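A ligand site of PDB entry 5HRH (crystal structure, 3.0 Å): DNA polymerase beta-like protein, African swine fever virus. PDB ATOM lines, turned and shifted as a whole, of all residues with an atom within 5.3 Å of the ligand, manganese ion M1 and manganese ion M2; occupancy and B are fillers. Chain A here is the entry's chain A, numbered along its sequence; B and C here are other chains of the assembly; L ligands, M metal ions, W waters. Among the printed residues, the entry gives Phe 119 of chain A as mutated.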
ATOM      1  N   VAL A  41      17.552 -19.258  19.525  1.00  0.00           N
ATOM      2  CA  VAL A  41      17.353 -17.832  19.357  1.00  0.00           C
ATOM      3  C   VAL A  41      16.014 -17.629  18.669  1.00  0.00           C
ATOM      4  O   VAL A  41      15.242 -18.580  18.464  1.00  0.00           O
ATOM      5  CB  VAL A  41      18.504 -17.120  18.590  1.00  0.00           C
ATOM      6  CG1 VAL A  41      19.778 -17.048  19.428  1.00  0.00           C
ATOM      7  CG2 VAL A  41      18.796 -17.788  17.242  1.00  0.00           C
ATOM      8  N   GLY A  42      15.711 -16.361  18.346  1.00  0.00           N
ATOM      9  CA  GLY A  42      14.436 -16.014  17.748  1.00  0.00           C
ATOM     10  C   GLY A  42      13.258 -16.127  18.709  1.00  0.00           C
ATOM     11  O   GLY A  42      13.386 -16.044  19.950  1.00  0.00           O
ATOM     12  N   SER A  43      12.072 -16.309  18.117  1.00  0.00           N
ATOM     13  CA  SER A  43      10.862 -16.343  18.919  1.00  0.00           C
ATOM     14  C   SER A  43      10.883 -17.460  19.947  1.00  0.00           C
ATOM     15  O   SER A  43      10.175 -17.370  20.943  1.00  0.00           O
ATOM     16  CB  SER A  43       9.634 -16.468  18.024  1.00  0.00           C
ATOM     17  OG  SER A  43       9.726 -17.582  17.151  1.00  0.00           O
ATOM     18  N   LEU A  44      11.695 -18.502  19.734  1.00  0.00           N
ATOM     19  CA  LEU A  44      11.820 -19.556  20.738  1.00  0.00           C
ATOM     20  C   LEU A  44      12.607 -19.070  21.960  1.00  0.00           C
ATOM     21  O   LEU A  44      12.253 -19.402  23.087  1.00  0.00           O
ATOM     22  CB  LEU A  44      12.476 -20.807  20.146  1.00  0.00           C
ATOM     23  CG  LEU A  44      12.423 -22.027  21.055  1.00  0.00           C
ATOM     24  CD1 LEU A  44      12.314 -23.254  20.225  1.00  0.00           C
ATOM     25  CD2 LEU A  44      13.643 -22.110  21.931  1.00  0.00           C
ATOM     26  N   ARG A  46      12.706 -16.014  22.834  1.00  0.00           N
ATOM     27  CA  ARG A  46      11.875 -14.975  23.425  1.00  0.00           C
ATOM     28  C   ARG A  46      10.583 -15.519  24.023  1.00  0.00           C
ATOM     29  O   ARG A  46       9.832 -14.761  24.638  1.00  0.00           O
ATOM     30  CB  ARG A  46      11.507 -13.901  22.388  1.00  0.00           C
ATOM     31  CG  ARG A  46      12.658 -13.076  21.845  1.00  0.00           C
ATOM     32  CD  ARG A  46      12.090 -11.822  21.222  1.00  0.00           C
ATOM     33  NE  ARG A  46      11.005 -12.155  20.300  1.00  0.00           N
ATOM     34  CZ  ARG A  46      11.131 -12.481  19.026  1.00  0.00           C
ATOM     35  NH1 ARG A  46      12.327 -12.462  18.462  1.00  0.00           N
ATOM     36  NH2 ARG A  46      10.054 -12.790  18.324  1.00  0.00           N
ATOM     37  N   MET A  50       3.599 -18.994  20.193  1.00  0.00           N
ATOM     38  CA  MET A  50       3.567 -19.689  18.917  1.00  0.00           C
ATOM     39  C   MET A  50       4.677 -19.176  18.005  1.00  0.00           C
ATOM     40  O   MET A  50       4.938 -17.993  17.915  1.00  0.00           O
ATOM     41  CB  MET A  50       2.187 -19.596  18.268  1.00  0.00           C
ATOM     42  N   LEU A  51       5.334 -20.119  17.348  1.00  0.00           N
ATOM     43  CA  LEU A  51       6.493 -19.892  16.487  1.00  0.00           C
ATOM     44  C   LEU A  51       6.103 -20.147  15.030  1.00  0.00           C
ATOM     45  O   LEU A  51       5.092 -20.791  14.749  1.00  0.00           O
ATOM     46  CB  LEU A  51       7.601 -20.863  16.921  1.00  0.00           C
ATOM     47  CG  LEU A  51       7.824 -21.048  18.436  1.00  0.00           C
ATOM     48  CD1 LEU A  51       8.779 -22.180  18.761  1.00  0.00           C
ATOM     49  CD2 LEU A  51       8.382 -19.783  19.046  1.00  0.00           C
ATOM     50  N   ASN A  52       6.906 -19.645  14.078  1.00  0.00           N
ATOM     51  CA  ASN A  52       6.736 -20.159  12.716  1.00  0.00           C
ATOM     52  C   ASN A  52       8.047 -20.605  12.091  1.00  0.00           C
ATOM     53  O   ASN A  52       8.098 -20.807  10.864  1.00  0.00           O
ATOM     54  CB  ASN A  52       6.033 -19.165  11.760  1.00  0.00           C
ATOM     55  CG  ASN A  52       6.550 -17.744  11.882  1.00  0.00           C
ATOM     56  OD1 ASN A  52       6.238 -17.039  12.821  1.00  0.00           O
ATOM     57  ND2 ASN A  52       7.316 -17.315  10.907  1.00  0.00           N
ATOM     58  N   ASP A  53       9.109 -20.758  12.879  1.00  0.00           N
ATOM     59  CA  ASP A  53      10.267 -21.584  12.564  1.00  0.00           C
ATOM     60  C   ASP A  53      11.101 -21.690  13.835  1.00  0.00           C
ATOM     61  O   ASP A  53      10.837 -21.006  14.830  1.00  0.00           O
ATOM     62  CB  ASP A  53      11.090 -21.032  11.378  1.00  0.00           C
ATOM     63  CG  ASP A  53      11.775 -19.695  11.676  1.00  0.00           C
ATOM     64  OD1 ASP A  53      11.496 -19.100  12.741  1.00  0.00           O
ATOM     65  OD2 ASP A  53      12.590 -19.227  10.843  1.00  0.00           O
ATOM     66  N   VAL A  54      12.098 -22.566  13.800  1.00  0.00           N
ATOM     67  CA  VAL A  54      13.134 -22.615  14.832  1.00  0.00           C
ATOM     68  C   VAL A  54      14.389 -21.977  14.275  1.00  0.00           C
ATOM     69  O   VAL A  54      14.779 -22.244  13.135  1.00  0.00           O
ATOM     70  CB  VAL A  54      13.410 -24.051  15.304  1.00  0.00           C
ATOM     71  CG1 VAL A  54      14.680 -24.083  16.125  1.00  0.00           C
ATOM     72  CG2 VAL A  54      12.278 -24.539  16.145  1.00  0.00           C
ATOM     73  N   ASP A  55      15.018 -21.112  15.075  1.00  0.00           N
ATOM     74  CA  ASP A  55      16.249 -20.444  14.690  1.00  0.00           C
ATOM     75  C   ASP A  55      17.326 -20.899  15.658  1.00  0.00           C
ATOM     76  O   ASP A  55      17.318 -20.485  16.833  1.00  0.00           O
ATOM     77  CB  ASP A  55      16.095 -18.915  14.727  1.00  0.00           C
ATOM     78  CG  ASP A  55      15.078 -18.395  13.730  1.00  0.00           C
ATOM     79  OD1 ASP A  55      14.973 -18.951  12.614  1.00  0.00           O
ATOM     80  OD2 ASP A  55      14.387 -17.391  14.086  1.00  0.00           O
ATOM     81  N   GLN A 102      10.116 -25.414   9.471  1.00  0.00           N
ATOM     82  CA  GLN A 102      11.272 -24.669   8.989  1.00  0.00           C
ATOM     83  C   GLN A 102      12.325 -24.481  10.082  1.00  0.00           C
ATOM     84  O   GLN A 102      12.034 -23.938  11.154  1.00  0.00           O
ATOM     85  CB  GLN A 102      10.838 -23.293   8.452  1.00  0.00           C
ATOM     86  CG  GLN A 102      11.979 -22.379   8.053  1.00  0.00           C
ATOM     87  CD  GLN A 102      11.493 -21.106   7.366  1.00  0.00           C
ATOM     88  OE1 GLN A 102      10.405 -21.070   6.791  1.00  0.00           O
ATOM     89  NE2 GLN A 102      12.277 -20.038   7.473  1.00  0.00           N
ATOM     90  N   ASP A 104      16.021 -22.655  10.674  1.00  0.00           N
ATOM     91  CA  ASP A 104      17.036 -21.717  10.203  1.00  0.00           C
ATOM     92  C   ASP A 104      18.269 -21.840  11.095  1.00  0.00           C
ATOM     93  O   ASP A 104      18.162 -21.710  12.315  1.00  0.00           O
ATOM     94  CB  ASP A 104      16.535 -20.279  10.198  1.00  0.00           C
ATOM     95  CG  ASP A 104      15.439 -20.077   9.197  1.00  0.00           C
ATOM     96  OD1 ASP A 104      15.227 -20.977   8.377  1.00  0.00           O
ATOM     97  OD2 ASP A 104      14.769 -19.019   9.238  1.00  0.00           O
ATOM     98  N   PHE A 106      22.308 -20.565  11.834  1.00  0.00           N
ATOM     99  CA  PHE A 106      23.282 -19.514  11.603  1.00  0.00           C
ATOM    100  C   PHE A 106      24.567 -19.881  12.306  1.00  0.00           C
ATOM    101  O   PHE A 106      24.624 -20.822  13.107  1.00  0.00           O
ATOM    102  CB  PHE A 106      22.777 -18.114  12.082  1.00  0.00           C
ATOM    103  CG  PHE A 106      21.431 -17.720  11.525  1.00  0.00           C
ATOM    104  CD1 PHE A 106      20.263 -18.325  11.977  1.00  0.00           C
ATOM    105  CD2 PHE A 106      21.378 -16.921  10.389  1.00  0.00           C
ATOM    106  CE1 PHE A 106      19.055 -18.000  11.418  1.00  0.00           C
ATOM    107  CE2 PHE A 106      20.184 -16.607   9.804  1.00  0.00           C
ATOM    108  CZ  PHE A 106      19.025 -17.149  10.316  1.00  0.00           C
ATOM    109  N   PHE A 119      21.588  -9.963  18.118  1.00  0.00           N
ATOM    110  CA  PHE A 119      20.969  -9.713  16.832  1.00  0.00           C
ATOM    111  C   PHE A 119      19.946 -10.811  16.476  1.00  0.00           C
ATOM    112  O   PHE A 119      18.866 -10.504  15.939  1.00  0.00           O
ATOM    113  CB  PHE A 119      22.063  -9.645  15.770  1.00  0.00           C
ATOM    114  CG  PHE A 119      21.560  -9.549  14.388  1.00  0.00           C
ATOM    115  CD1 PHE A 119      21.209  -8.307  13.865  1.00  0.00           C
ATOM    116  CD2 PHE A 119      21.319 -10.701  13.636  1.00  0.00           C
ATOM    117  CE1 PHE A 119      20.716  -8.194  12.568  1.00  0.00           C
ATOM    118  CE2 PHE A 119      20.802 -10.614  12.346  1.00  0.00           C
ATOM    119  CZ  PHE A 119      20.508  -9.362  11.810  1.00  0.00           C
ATOM    120  N   PHE A 120      20.245 -12.083  16.782  1.00  0.00           N
ATOM    121  CA  PHE A 120      19.415 -13.206  16.333  1.00  0.00           C
ATOM    122  C   PHE A 120      18.331 -13.642  17.303  1.00  0.00           C
ATOM    123  O   PHE A 120      17.548 -14.544  16.951  1.00  0.00           O
ATOM    124  CB  PHE A 120      20.280 -14.441  15.995  1.00  0.00           C
ATOM    125  CG  PHE A 120      20.901 -14.366  14.639  1.00  0.00           C
ATOM    126  CD1 PHE A 120      20.104 -14.390  13.516  1.00  0.00           C
ATOM    127  CD2 PHE A 120      22.268 -14.268  14.493  1.00  0.00           C
ATOM    128  CE1 PHE A 120      20.650 -14.288  12.280  1.00  0.00           C
ATOM    129  CE2 PHE A 120      22.830 -14.166  13.240  1.00  0.00           C
ATOM    130  CZ  PHE A 120      22.028 -14.169  12.140  1.00  0.00           C
ATOM    131  N   THR A 121      18.251 -13.094  18.534  1.00  0.00           N
ATOM    132  CA  THR A 121      17.013 -13.331  19.298  1.00  0.00           C
ATOM    133  C   THR A 121      15.914 -12.357  18.866  1.00  0.00           C
ATOM    134  O   THR A 121      14.755 -12.751  18.710  1.00  0.00           O
ATOM    135  CB  THR A 121      17.216 -13.237  20.821  1.00  0.00           C
ATOM    136  OG1 THR A 121      17.384 -11.883  21.220  1.00  0.00           O
ATOM    137  CG2 THR A 121      18.459 -13.908  21.178  1.00  0.00           C
ATOM    138  N   GLY A 122      16.272 -11.100  18.626  1.00  0.00           N
ATOM    139  CA  GLY A 122      15.290 -10.097  18.290  1.00  0.00           C
ATOM    140  C   GLY A 122      14.619  -9.419  19.477  1.00  0.00           C
ATOM    141  O   GLY A 122      15.280  -9.166  20.503  1.00  0.00           O
ATOM    142  N   PRO A 123      13.329  -9.054  19.318  1.00  0.00           N
ATOM    143  CA  PRO A 123      12.520  -9.169  18.082  1.00  0.00           C
ATOM    144  C   PRO A 123      13.012  -8.187  16.995  1.00  0.00           C
ATOM    145  O   PRO A 123      13.973  -7.475  17.221  1.00  0.00           O
ATOM    146  CB  PRO A 123      11.110  -8.847  18.557  1.00  0.00           C
ATOM    147  CG  PRO A 123      11.308  -7.974  19.703  1.00  0.00           C
ATOM    148  CD  PRO A 123      12.567  -8.400  20.395  1.00  0.00           C
ATOM    149  N   VAL A 124      12.382  -8.185  15.819  1.00  0.00           N
ATOM    150  CA  VAL A 124      12.898  -7.347  14.728  1.00  0.00           C
ATOM    151  C   VAL A 124      12.895  -5.869  15.116  1.00  0.00           C
ATOM    152  O   VAL A 124      13.916  -5.180  15.019  1.00  0.00           O
ATOM    153  CB  VAL A 124      12.091  -7.581  13.446  1.00  0.00           C
ATOM    154  CG1 VAL A 124      12.809  -7.013  12.275  1.00  0.00           C
ATOM    155  CG2 VAL A 124      11.773  -9.060  13.296  1.00  0.00           C
ATOM    156  N   LEU A 127      15.511  -4.551  17.155  1.00  0.00           N
ATOM    157  CA  LEU A 127      16.783  -4.404  16.454  1.00  0.00           C
ATOM    158  C   LEU A 127      16.807  -3.138  15.636  1.00  0.00           C
ATOM    159  O   LEU A 127      17.809  -2.405  15.640  1.00  0.00           O
ATOM    160  CB  LEU A 127      17.014  -5.597  15.527  1.00  0.00           C
ATOM    161  CG  LEU A 127      17.809  -6.785  16.030  1.00  0.00           C
ATOM    162  CD1 LEU A 127      17.196  -7.308  17.272  1.00  0.00           C
ATOM    163  CD2 LEU A 127      17.747  -7.827  14.925  1.00  0.00           C
ATOM    164  P    DG B   9      17.299   3.601   9.862  1.00  0.00           P
ATOM    165  OP1  DG B   9      18.518   4.315   9.411  1.00  0.00           O
ATOM    166  OP2  DG B   9      16.440   2.789   8.948  1.00  0.00           O
ATOM    167  O5'  DG B   9      17.930   2.702  11.004  1.00  0.00           O
ATOM    168  C5'  DG B   9      17.547   1.368  11.187  1.00  0.00           C
ATOM    169  C4'  DG B   9      18.793   0.559  11.423  1.00  0.00           C
ATOM    170  O4'  DG B   9      18.478  -0.835  11.384  1.00  0.00           O
ATOM    171  C3'  DG B   9      19.869   0.759  10.365  1.00  0.00           C
ATOM    172  O3'  DG B   9      21.170   0.492  10.911  1.00  0.00           O
ATOM    173  C2'  DG B   9      19.435  -0.242   9.280  1.00  0.00           C
ATOM    174  C1'  DG B   9      18.793  -1.363  10.113  1.00  0.00           C
ATOM    175  N9   DG B   9      17.574  -1.946   9.569  1.00  0.00           N
ATOM    176  C8   DG B   9      16.516  -1.305   8.976  1.00  0.00           C
ATOM    177  N7   DG B   9      15.549  -2.120   8.635  1.00  0.00           N
ATOM    178  C5   DG B   9      15.991  -3.367   9.030  1.00  0.00           C
ATOM    179  C6   DG B   9      15.382  -4.643   8.907  1.00  0.00           C
ATOM    180  O6   DG B   9      14.281  -4.921   8.406  1.00  0.00           O
ATOM    181  N1   DG B   9      16.196  -5.657   9.451  1.00  0.00           N
ATOM    182  C2   DG B   9      17.436  -5.435  10.032  1.00  0.00           C
ATOM    183  N2   DG B   9      18.082  -6.499  10.493  1.00  0.00           N
ATOM    184  N3   DG B   9      18.002  -4.257  10.150  1.00  0.00           N
ATOM    185  C4   DG B   9      17.233  -3.277   9.623  1.00  0.00           C
ATOM    186  P    DT B  10      22.486   0.537   9.979  1.00  0.00           P
ATOM    187  OP1  DT B  10      23.671   0.858  10.832  1.00  0.00           O
ATOM    188  OP2  DT B  10      22.262   1.411   8.799  1.00  0.00           O
ATOM    189  O5'  DT B  10      22.570  -0.973   9.464  1.00  0.00           O
ATOM    190  C5'  DT B  10      22.666  -2.021  10.408  1.00  0.00           C
ATOM    191  C4'  DT B  10      22.642  -3.342   9.699  1.00  0.00           C
ATOM    192  O4'  DT B  10      21.321  -3.647   9.273  1.00  0.00           O
ATOM    193  C3'  DT B  10      23.477  -3.349   8.444  1.00  0.00           C
ATOM    194  O3'  DT B  10      24.739  -3.865   8.767  1.00  0.00           O
ATOM    195  C2'  DT B  10      22.696  -4.271   7.455  1.00  0.00           C
ATOM    196  C1'  DT B  10      21.379  -4.539   8.185  1.00  0.00           C
ATOM    197  N1   DT B  10      20.154  -4.336   7.398  1.00  0.00           N
ATOM    198  C2   DT B  10      19.325  -5.400   7.175  1.00  0.00           C
ATOM    199  O2   DT B  10      19.557  -6.525   7.577  1.00  0.00           O
ATOM    200  N3   DT B  10      18.169  -5.097   6.490  1.00  0.00           N
ATOM    201  C4   DT B  10      17.797  -3.853   6.027  1.00  0.00           C
ATOM    202  O4   DT B  10      16.751  -3.676   5.401  1.00  0.00           O
ATOM    203  C5   DT B  10      18.721  -2.782   6.300  1.00  0.00           C
ATOM    204  C7   DT B  10      18.420  -1.412   5.824  1.00  0.00           C
ATOM    205  C6   DT B  10      19.839  -3.071   6.976  1.00  0.00           C
ATOM    206  P    DA C   9      11.582 -15.630   5.928  1.00  0.00           P
ATOM    207  OP1  DA C   9      12.116 -16.590   6.926  1.00  0.00           O
ATOM    208  OP2  DA C   9      10.385 -15.984   5.128  1.00  0.00           O
ATOM    209  O5'  DA C   9      11.298 -14.238   6.663  1.00  0.00           O
ATOM    210  C5'  DA C   9      12.118 -13.807   7.757  1.00  0.00           C
ATOM    211  C4'  DA C   9      13.583 -14.047   7.452  1.00  0.00           C
ATOM    212  O4'  DA C   9      14.028 -13.055   6.492  1.00  0.00           O
ATOM    213  C3'  DA C   9      14.515 -13.924   8.652  1.00  0.00           C
ATOM    214  C2'  DA C   9      15.020 -12.490   8.550  1.00  0.00           C
ATOM    215  C1'  DA C   9      15.076 -12.269   7.047  1.00  0.00           C
ATOM    216  N9   DA C   9      14.866 -10.886   6.627  1.00  0.00           N
ATOM    217  C8   DA C   9      13.710 -10.323   6.125  1.00  0.00           C
ATOM    218  N7   DA C   9      13.831  -9.053   5.846  1.00  0.00           N
ATOM    219  C5   DA C   9      15.145  -8.749   6.189  1.00  0.00           C
ATOM    220  C6   DA C   9      15.885  -7.563   6.121  1.00  0.00           C
ATOM    221  N6   DA C   9      15.396  -6.403   5.677  1.00  0.00           N
ATOM    222  N1   DA C   9      17.175  -7.601   6.542  1.00  0.00           N
ATOM    223  C2   DA C   9      17.664  -8.761   6.987  1.00  0.00           C
ATOM    224  N3   DA C   9      17.060  -9.944   7.094  1.00  0.00           N
ATOM    225  C4   DA C   9      15.789  -9.874   6.674  1.00  0.00           C
HETATM  226  P1  LIG L   1       9.310 -16.074  14.272  1.00  0.00           P
HETATM  227  O1  LIG L   1       8.602 -15.307  13.207  1.00  0.00           O
HETATM  228  O2  LIG L   1       8.347 -17.007  14.966  1.00  0.00           O
HETATM  229  O3  LIG L   1      10.384 -16.939  13.677  1.00  0.00           O
HETATM  230  O4  LIG L   1       9.947 -15.007  15.281  1.00  0.00           O
HETATM  231  P2  LIG L   1      11.452 -14.613  14.986  1.00  0.00           P
HETATM  232  O5  LIG L   1      12.285 -15.836  15.253  1.00  0.00           O
HETATM  233  O6  LIG L   1      11.976 -13.382  15.679  1.00  0.00           O
HETATM  234  O7  LIG L   1      11.347 -14.456  13.400  1.00  0.00           O
HETATM  235  P3  LIG L   1      12.532 -14.918  12.411  1.00  0.00           P
HETATM  236  O8  LIG L   1      12.458 -16.409  12.133  1.00  0.00           O
HETATM  237  O9  LIG L   1      12.461 -14.071  11.156  1.00  0.00           O
HETATM  238  O10 LIG L   1      13.830 -14.529  13.274  1.00  0.00           O
HETATM  239  C1  LIG L   1      14.977 -14.174  12.581  1.00  0.00           C
HETATM  240  C2  LIG L   1      15.878 -13.418  13.519  1.00  0.00           C
HETATM  241  O11 LIG L   1      16.694 -12.664  12.657  1.00  0.00           O
HETATM  242  C3  LIG L   1      15.085 -12.457  14.351  1.00  0.00           C
HETATM  243  O12 LIG L   1      14.944 -12.907  15.671  1.00  0.00           O
HETATM  244  C4  LIG L   1      15.916 -11.188  14.339  1.00  0.00           C
HETATM  245  C5  LIG L   1      16.789 -11.332  13.099  1.00  0.00           C
HETATM  246  N1  LIG L   1      16.381 -10.371  12.071  1.00  0.00           N
HETATM  247  C6  LIG L   1      17.237  -9.437  11.560  1.00  0.00           C
HETATM  248  N2  LIG L   1      16.594  -8.703  10.623  1.00  0.00           N
HETATM  249  C7  LIG L   1      15.340  -9.160  10.530  1.00  0.00           C
HETATM  250  C8  LIG L   1      14.314  -8.718   9.738  1.00  0.00           C
HETATM  251  O13 LIG L   1      14.543  -7.752   8.979  1.00  0.00           O
HETATM  252  N3  LIG L   1      13.091  -9.378   9.808  1.00  0.00           N
HETATM  253  C9  LIG L   1      12.947 -10.430  10.681  1.00  0.00           C
HETATM  254  N4  LIG L   1      11.771 -11.059  10.774  1.00  0.00           N
HETATM  255  N5  LIG L   1      13.989 -10.848  11.494  1.00  0.00           N
HETATM  256  C10 LIG L   1      15.183 -10.218  11.414  1.00  0.00           C
HETATM  257 MN    MN M   1      12.041 -17.800  14.215  1.00  0.00          MN
HETATM  258 MN    MN M   2      14.181 -17.502  10.920  1.00  0.00          MN
HETATM  259  O   HOH W   1      11.953 -19.222  15.800  1.00  0.00           O
HETATM  260  O   HOH W   2      12.721 -16.720   9.621  1.00  0.00           O
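Residues that only touch manganese ion M1: Ser 43 (3.7 Å).
N2 of DG 9 of chain B sits close to N2 of the ligand, at 2.7 Å.
The guanidinium group (NH1) of Arg 46 lies within salt-bridge range of an oxygen (O6) of the ligand, 3.0 Å away.
The backbone NH (N) of Asn 52 lies within hydrogen-bond range of an oxygen (O2) of the ligand (3.1 Å).
The side-chain amide oxygen (OD1) of Asn 52 lies close to an oxygen (O1) of the ligand, at 3.0 Å.
OG of Ser 43 sits at hydrogen-bond distance from O2 of the ligand (2.6 Å).
The backbone NH (N) of Ser 43 sits close to an oxygen (O5) of the ligand, at 2.9 Å.
O of Phe 120 sits at hydrogen-bond distance from O12 of the ligand (3.3 Å).
The backbone carbonyl oxygen (O) of Thr 121 is in hydrogen-bond range of an oxygen (O12) of the ligand (3.0 Å).
N7 of DA 9 of chain C lies close to an oxygen (O13) of the ligand (3.5 Å).
Gly 42 touches the ligand.
Leu 51 touches the ligand (CA to O2, 3.8 Å).
Phe 119 touches the ligand.
Gly 122 touches the ligand (N to O12, 3.7 Å).
Val 124 touches the ligand.
CD2 of Leu 127 touches C6 of the ligand, 3.8 Å away.
Of the 24 residues printed, 15 come within 4 Å of the ligand.
The nearest printed residue that does not touch the ligand is Asp 104 (4.5 Å).
N1 of DA 9 of chain C lies close to N3 of DT 10 of chain B (2.7 Å).
The side-chain carboxylate (OD2) of Asp 53 sits close to the side-chain amide nitrogen (NE2) of Gln 102 (3.5 Å).
OP1 of DA 9 of chain C sits at hydrogen-bond distance from the side-chain amide nitrogen of Gln 102 (3.5 Å).
O of Asp 55 sits at hydrogen-bond distance from N of Val 41 (3.0 Å).
The backbone NH (N) of Asp 104 lies within hydrogen-bond range of the backbone carbonyl oxygen (O) of Val 54 (2.8 Å).
The backbone carbonyl oxygen (O) of Phe 120 sits at hydrogen-bond distance from the backbone NH (N) of Gly 42 (2.9 Å).
The side-chain amide nitrogen (NE2) of Gln 102 lies within hydrogen-bond range of the side-chain carboxylate (OD1) of Asp 104, 3.2 Å away.
The guanidinium group (NH1) of Arg 46 sits at hydrogen-bond distance from the backbone carbonyl oxygen (O) of Thr 121, 2.5 Å away.
Water W2 lies within hydrogen-bond range of OP1 of DA 9 of chain C and an oxygen (O9) of the ligand.
Manganese ion M1 is bound by O3 of the ligand (1.9 Å), OD1 of Asp 53 (2.0 Å), water W1 (2.1 Å), O5 of the ligand (2.2 Å), OD2 of Asp 55 (2.4 Å) and O8 of the ligand (2.5 Å).
Manganese ion M1 has six donor atoms within binding distance.
Within 4 Å of manganese ion M2: Asp 53, Asp 55 and Asp 104.
Manganese ion M2 is bound by water W2 (2.1 Å), OD2 of Asp 104 (2.3 Å), OD2 of Asp 53 (2.3 Å), OD1 of Asp 55 (2.4 Å) and O8 of the ligand (2.4 Å).
Manganese ion M2 has five donor atoms within binding distance.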
